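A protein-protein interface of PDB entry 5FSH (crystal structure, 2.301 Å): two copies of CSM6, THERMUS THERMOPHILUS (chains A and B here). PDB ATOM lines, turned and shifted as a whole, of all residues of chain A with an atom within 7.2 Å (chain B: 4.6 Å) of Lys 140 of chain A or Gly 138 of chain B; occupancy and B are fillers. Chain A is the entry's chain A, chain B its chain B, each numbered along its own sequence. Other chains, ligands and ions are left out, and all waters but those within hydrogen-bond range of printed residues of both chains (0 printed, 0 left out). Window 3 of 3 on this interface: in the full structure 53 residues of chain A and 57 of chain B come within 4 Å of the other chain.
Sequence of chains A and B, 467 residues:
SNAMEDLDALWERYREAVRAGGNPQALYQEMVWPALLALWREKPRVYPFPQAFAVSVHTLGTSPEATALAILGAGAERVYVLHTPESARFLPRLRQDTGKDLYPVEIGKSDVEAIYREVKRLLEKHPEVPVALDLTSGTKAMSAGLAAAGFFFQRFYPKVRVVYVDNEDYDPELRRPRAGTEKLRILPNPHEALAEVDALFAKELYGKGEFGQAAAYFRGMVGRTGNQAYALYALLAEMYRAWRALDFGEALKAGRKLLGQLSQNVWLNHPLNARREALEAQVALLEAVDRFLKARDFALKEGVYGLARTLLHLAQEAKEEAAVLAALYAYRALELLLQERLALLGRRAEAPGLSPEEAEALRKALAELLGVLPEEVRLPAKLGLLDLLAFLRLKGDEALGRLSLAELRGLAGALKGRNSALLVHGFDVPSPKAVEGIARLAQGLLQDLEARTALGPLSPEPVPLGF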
ATOM      1  N   LYS A 109      -5.685 -22.087 -22.489  1.00  0.00           N
ATOM      2  CA  LYS A 109      -5.413 -20.837 -21.786  1.00  0.00           C
ATOM      3  C   LYS A 109      -4.029 -20.799 -21.140  1.00  0.00           C
ATOM      4  O   LYS A 109      -3.484 -19.707 -20.942  1.00  0.00           O
ATOM      5  CB  LYS A 109      -6.487 -20.586 -20.730  1.00  0.00           C
ATOM      6  CG  LYS A 109      -7.756 -19.962 -21.281  1.00  0.00           C
ATOM      7  CD  LYS A 109      -8.360 -18.968 -20.298  1.00  0.00           C
ATOM      8  CE  LYS A 109      -9.298 -17.990 -21.000  1.00  0.00           C
ATOM      9  NZ  LYS A 109      -8.897 -16.563 -20.788  1.00  0.00           N
ATOM     10  N   VAL A 112       1.435 -22.163 -23.371  1.00  0.00           N
ATOM     11  CA  VAL A 112       2.399 -21.237 -23.961  1.00  0.00           C
ATOM     12  C   VAL A 112       3.161 -21.914 -25.088  1.00  0.00           C
ATOM     13  O   VAL A 112       3.447 -21.298 -26.127  1.00  0.00           O
ATOM     14  CB  VAL A 112       3.360 -20.697 -22.884  1.00  0.00           C
ATOM     15  CG1 VAL A 112       4.458 -19.843 -23.526  1.00  0.00           C
ATOM     16  CG2 VAL A 112       2.594 -19.906 -21.848  1.00  0.00           C
ATOM     17  N   GLY A 138      -6.245 -11.997 -23.830  1.00  0.00           N
ATOM     18  CA  GLY A 138      -5.720 -13.279 -23.398  1.00  0.00           C
ATOM     19  C   GLY A 138      -5.205 -13.287 -21.971  1.00  0.00           C
ATOM     20  O   GLY A 138      -5.130 -12.239 -21.327  1.00  0.00           O
ATOM     21  N   THR A 139      -4.859 -14.465 -21.456  1.00  0.00           N
ATOM     22  CA  THR A 139      -4.231 -14.570 -20.146  1.00  0.00           C
ATOM     23  C   THR A 139      -2.811 -14.010 -20.196  1.00  0.00           C
ATOM     24  O   THR A 139      -2.211 -13.870 -21.265  1.00  0.00           O
ATOM     25  CB  THR A 139      -4.197 -16.025 -19.678  1.00  0.00           C
ATOM     26  OG1 THR A 139      -3.232 -16.751 -20.446  1.00  0.00           O
ATOM     27  CG2 THR A 139      -5.552 -16.675 -19.881  1.00  0.00           C
ATOM     28  N   LYS A 140      -2.271 -13.688 -19.015  1.00  0.00           N
ATOM     29  CA  LYS A 140      -0.901 -13.179 -18.955  1.00  0.00           C
ATOM     30  C   LYS A 140       0.063 -14.119 -19.661  1.00  0.00           C
ATOM     31  O   LYS A 140       0.996 -13.678 -20.339  1.00  0.00           O
ATOM     32  CB  LYS A 140      -0.462 -12.982 -17.508  1.00  0.00           C
ATOM     33  CG  LYS A 140      -1.216 -11.906 -16.763  1.00  0.00           C
ATOM     34  CD  LYS A 140      -0.978 -10.530 -17.354  1.00  0.00           C
ATOM     35  CE  LYS A 140      -1.165  -9.475 -16.274  1.00  0.00           C
ATOM     36  NZ  LYS A 140      -1.539  -8.147 -16.818  1.00  0.00           N
ATOM     37  N   ALA A 141      -0.161 -15.422 -19.527  1.00  0.00           N
ATOM     38  CA  ALA A 141       0.732 -16.398 -20.141  1.00  0.00           C
ATOM     39  C   ALA A 141       0.631 -16.359 -21.658  1.00  0.00           C
ATOM     40  O   ALA A 141       1.646 -16.463 -22.356  1.00  0.00           O
ATOM     41  CB  ALA A 141       0.421 -17.799 -19.609  1.00  0.00           C
ATOM     42  N   MET A 142      -0.586 -16.199 -22.190  1.00  0.00           N
ATOM     43  CA  MET A 142      -0.750 -16.126 -23.639  1.00  0.00           C
ATOM     44  C   MET A 142      -0.113 -14.864 -24.206  1.00  0.00           C
ATOM     45  O   MET A 142       0.596 -14.923 -25.217  1.00  0.00           O
ATOM     46  CB  MET A 142      -2.235 -16.179 -24.025  1.00  0.00           C
ATOM     47  CG  MET A 142      -2.941 -17.504 -23.760  1.00  0.00           C
ATOM     48  SD  MET A 142      -4.704 -17.435 -24.179  1.00  0.00           S
ATOM     49  CE  MET A 142      -4.629 -17.074 -25.929  1.00  0.00           C
ATOM     50  N   SER A 143      -0.363 -13.711 -23.572  1.00  0.00           N
ATOM     51  CA  SER A 143       0.155 -12.443 -24.085  1.00  0.00           C
ATOM     52  C   SER A 143       1.672 -12.378 -23.977  1.00  0.00           C
ATOM     53  O   SER A 143       2.358 -12.001 -24.934  1.00  0.00           O
ATOM     54  CB  SER A 143      -0.467 -11.272 -23.330  1.00  0.00           C
ATOM     55  OG  SER A 143      -1.861 -11.208 -23.522  1.00  0.00           O
ATOM     56  N   ALA A 144       2.211 -12.704 -22.800  1.00  0.00           N
ATOM     57  CA  ALA A 144       3.657 -12.704 -22.619  1.00  0.00           C
ATOM     58  C   ALA A 144       4.319 -13.718 -23.539  1.00  0.00           C
ATOM     59  O   ALA A 144       5.400 -13.465 -24.082  1.00  0.00           O
ATOM     60  CB  ALA A 144       4.006 -13.007 -21.162  1.00  0.00           C
ATOM     61  N   GLY A 145       3.684 -14.875 -23.728  1.00  0.00           N
ATOM     62  CA  GLY A 145       4.206 -15.835 -24.682  1.00  0.00           C
ATOM     63  C   GLY A 145       4.240 -15.293 -26.097  1.00  0.00           C
ATOM     64  O   GLY A 145       5.206 -15.520 -26.830  1.00  0.00           O
ATOM     65  N   LEU A 146       3.193 -14.568 -26.502  1.00  0.00           N
ATOM     66  CA  LEU A 146       3.178 -13.994 -27.845  1.00  0.00           C
ATOM     67  C   LEU A 146       4.272 -12.941 -28.004  1.00  0.00           C
ATOM     68  O   LEU A 146       4.958 -12.898 -29.031  1.00  0.00           O
ATOM     69  CB  LEU A 146       1.806 -13.392 -28.163  1.00  0.00           C
ATOM     70  CG  LEU A 146       1.547 -13.171 -29.661  1.00  0.00           C
ATOM     71  CD1 LEU A 146       1.153 -14.475 -30.357  1.00  0.00           C
ATOM     72  CD2 LEU A 146       0.490 -12.107 -29.904  1.00  0.00           C
ATOM     73  N   LEU B  60       3.400  -4.753 -10.541  1.00  0.00           N
ATOM     74  CA  LEU B  60       2.211  -4.612  -9.710  1.00  0.00           C
ATOM     75  C   LEU B  60       1.185  -3.754 -10.433  1.00  0.00           C
ATOM     76  O   LEU B  60       1.449  -2.583 -10.726  1.00  0.00           O
ATOM     77  CB  LEU B  60       2.556  -4.000  -8.351  1.00  0.00           C
ATOM     78  CG  LEU B  60       1.392  -3.933  -7.361  1.00  0.00           C
ATOM     79  CD1 LEU B  60       0.798  -5.312  -7.132  1.00  0.00           C
ATOM     80  CD2 LEU B  60       1.851  -3.327  -6.049  1.00  0.00           C
ATOM     81  N   GLY B  61       0.019  -4.338 -10.709  1.00  0.00           N
ATOM     82  CA  GLY B  61      -1.089  -3.630 -11.318  1.00  0.00           C
ATOM     83  C   GLY B  61      -2.252  -3.440 -10.362  1.00  0.00           C
ATOM     84  O   GLY B  61      -2.182  -2.592  -9.465  1.00  0.00           O
ATOM     85  N   LEU B 135       5.524 -11.719 -13.668  1.00  0.00           N
ATOM     86  CA  LEU B 135       4.727 -10.853 -14.525  1.00  0.00           C
ATOM     87  C   LEU B 135       3.234 -10.928 -14.225  1.00  0.00           C
ATOM     88  O   LEU B 135       2.432 -10.385 -14.995  1.00  0.00           O
ATOM     89  CB  LEU B 135       4.996 -11.200 -15.990  1.00  0.00           C
ATOM     90  CG  LEU B 135       4.814 -12.662 -16.431  1.00  0.00           C
ATOM     91  CD1 LEU B 135       3.338 -13.050 -16.598  1.00  0.00           C
ATOM     92  CD2 LEU B 135       5.579 -12.919 -17.716  1.00  0.00           C
ATOM     93  N   THR B 136       2.845 -11.576 -13.120  1.00  0.00           N
ATOM     94  CA  THR B 136       1.437 -11.900 -12.894  1.00  0.00           C
ATOM     95  C   THR B 136       0.544 -10.664 -12.900  1.00  0.00           C
ATOM     96  O   THR B 136      -0.570 -10.700 -13.433  1.00  0.00           O
ATOM     97  CB  THR B 136       1.276 -12.638 -11.572  1.00  0.00           C
ATOM     98  OG1 THR B 136       2.161 -13.766 -11.545  1.00  0.00           O
ATOM     99  CG2 THR B 136      -0.170 -13.107 -11.403  1.00  0.00           C
ATOM    100  N   SER B 137       0.997  -9.571 -12.300  1.00  0.00           N
ATOM    101  CA  SER B 137       0.172  -8.382 -12.155  1.00  0.00           C
ATOM    102  C   SER B 137       0.765  -7.224 -12.933  1.00  0.00           C
ATOM    103  O   SER B 137       1.986  -7.114 -13.071  1.00  0.00           O
ATOM    104  CB  SER B 137       0.041  -8.003 -10.671  1.00  0.00           C
ATOM    105  OG  SER B 137      -0.598  -6.750 -10.516  1.00  0.00           O
ATOM    106  N   GLY B 138      -0.119  -6.363 -13.440  1.00  0.00           N
ATOM    107  CA  GLY B 138       0.279  -5.239 -14.256  1.00  0.00           C
ATOM    108  C   GLY B 138      -0.553  -5.149 -15.517  1.00  0.00           C
ATOM    109  O   GLY B 138      -1.347  -6.030 -15.846  1.00  0.00           O
ATOM    110  N   THR B 139      -0.358  -4.039 -16.234  1.00  0.00           N
ATOM    111  CA  THR B 139      -0.946  -3.920 -17.562  1.00  0.00           C
ATOM    112  C   THR B 139      -0.326  -4.944 -18.506  1.00  0.00           C
ATOM    113  O   THR B 139       0.716  -5.541 -18.223  1.00  0.00           O
ATOM    114  CB  THR B 139      -0.740  -2.515 -18.124  1.00  0.00           C
ATOM    115  OG1 THR B 139       0.660  -2.295 -18.348  1.00  0.00           O
ATOM    116  CG2 THR B 139      -1.241  -1.465 -17.145  1.00  0.00           C
ATOM    117  N   LYS B 140      -0.976  -5.131 -19.651  1.00  0.00           N
ATOM    118  CA  LYS B 140      -0.435  -6.039 -20.658  1.00  0.00           C
ATOM    119  C   LYS B 140       0.948  -5.595 -21.115  1.00  0.00           C
ATOM    120  O   LYS B 140       1.838  -6.425 -21.340  1.00  0.00           O
ATOM    121  CB  LYS B 140      -1.399  -6.150 -21.848  1.00  0.00           C
ATOM    122  CG  LYS B 140      -2.594  -7.059 -21.556  1.00  0.00           C
ATOM    123  CD  LYS B 140      -2.122  -8.488 -21.283  1.00  0.00           C
ATOM    124  CE  LYS B 140      -3.222  -9.377 -20.728  1.00  0.00           C
ATOM    125  NZ  LYS B 140      -4.349  -9.508 -21.681  1.00  0.00           N
ATOM    126  N   MET B 142       3.147  -3.936 -19.277  1.00  0.00           N
ATOM    127  CA  MET B 142       4.099  -4.183 -18.197  1.00  0.00           C
ATOM    128  C   MET B 142       4.518  -5.647 -18.148  1.00  0.00           C
ATOM    129  O   MET B 142       5.712  -5.959 -18.087  1.00  0.00           O
ATOM    130  CB  MET B 142       3.501  -3.756 -16.855  1.00  0.00           C
ATOM    131  CG  MET B 142       3.303  -2.261 -16.722  1.00  0.00           C
ATOM    132  SD  MET B 142       2.340  -1.803 -15.266  1.00  0.00           S
ATOM    133  CE  MET B 142       3.501  -2.189 -13.950  1.00  0.00           C
ATOM    134  N   SER B 143       3.543  -6.559 -18.162  1.00  0.00           N
ATOM    135  CA  SER B 143       3.848  -7.985 -18.099  1.00  0.00           C
ATOM    136  C   SER B 143       4.617  -8.439 -19.330  1.00  0.00           C
ATOM    137  O   SER B 143       5.634  -9.141 -19.218  1.00  0.00           O
ATOM    138  CB  SER B 143       2.558  -8.787 -17.956  1.00  0.00           C
ATOM    139  OG  SER B 143       1.856  -8.400 -16.797  1.00  0.00           O
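The side-chain amino group (NZ) of Lys 140 of chain A lies close to the side-chain hydroxyl (OG) of Ser 143 of chain B (3.4 Å).
O of Gly 138 of chain A is in hydrogen-bond range of NZ of Lys 140 of chain B (2.9 Å).
NZ of Lys 140 of chain A sits close to O of Gly 138 of chain B (2.3 Å).
The backbone NH of Met 142 of chain B sits close to the side-chain hydroxyl of Thr 139 of chain B, 3.1 Å away.
OG of Ser 143 of chain B sits at hydrogen-bond distance from O of Leu 135 of chain B (2.7 Å).
O of Thr 139 of chain B is in hydrogen-bond range of OG of Ser 143 of chain B (3.4 Å).
Lys 140 of chain A touches Leu 135 of chain B (CB to CD1, 3.9 Å).
Lys 140 of chain A touches Thr 136 of chain B (CE to O, 3.2 Å).
Lys 140 of chain A touches Thr 139 of chain B.
OG of Ser 143 of chain A touches NZ of Lys 140 of chain B (3.5 Å).
Ala 144 of chain A touches Leu 135 of chain B.
Of chain B, only Leu 135 (3.9 Å), Thr 136 (3.2 Å), Gly 138 (2.3 Å), Thr 139 (3.7 Å) and Ser 143 (3.2 Å) come within 4 Å of Lys 140 of chain A.
Of chain A, only Lys 140 comes within 4 Å of Gly 138 of chain B.
Of the printed residues of chain B, Ser 143 of chain A touches Lys 140.
Of the printed residues of chain A, Thr 139 of chain B touches Lys 140 (3.7 Å).
Of the printed residues of chain B, Gly 138 of chain A touches Lys 140.
Leu 60 of chain B touches none of the printed residues of chain A.
The nearest printed residue of chain A that does not touch Gly 138 of chain B is Gly 138 of chain A (9.1 Å).
Of the 10 printed residues of chain B, 6 touch a printed residue of chain A.
Among the printed residues, 8 pairs touch across the chains.
Among the printed residues, no Asp or Glu carboxylate lies within 4 Å of a Lys or Arg side-chain nitrogen of the other chain.
Gly 138 of chain A touches Lys 140 of chain B, and with the chains exchanged Lys 140 of chain A touches Gly 138 of chain B.
Lys 140 of chain A touches Thr 139 of chain B, but with the chains exchanged Thr 139 of chain A does not touch Lys 140 of chain B (4.6 Å).
Lys 140 of chain A touches Ser 143 of chain B, and with the chains exchanged Ser 143 of chain A touches Lys 140 of chain B.
5 positions are printed for both chains.
Of the 8 pairs that touch across the chains among the printed residues, 4 have their exchanged pair printed and touching as well.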
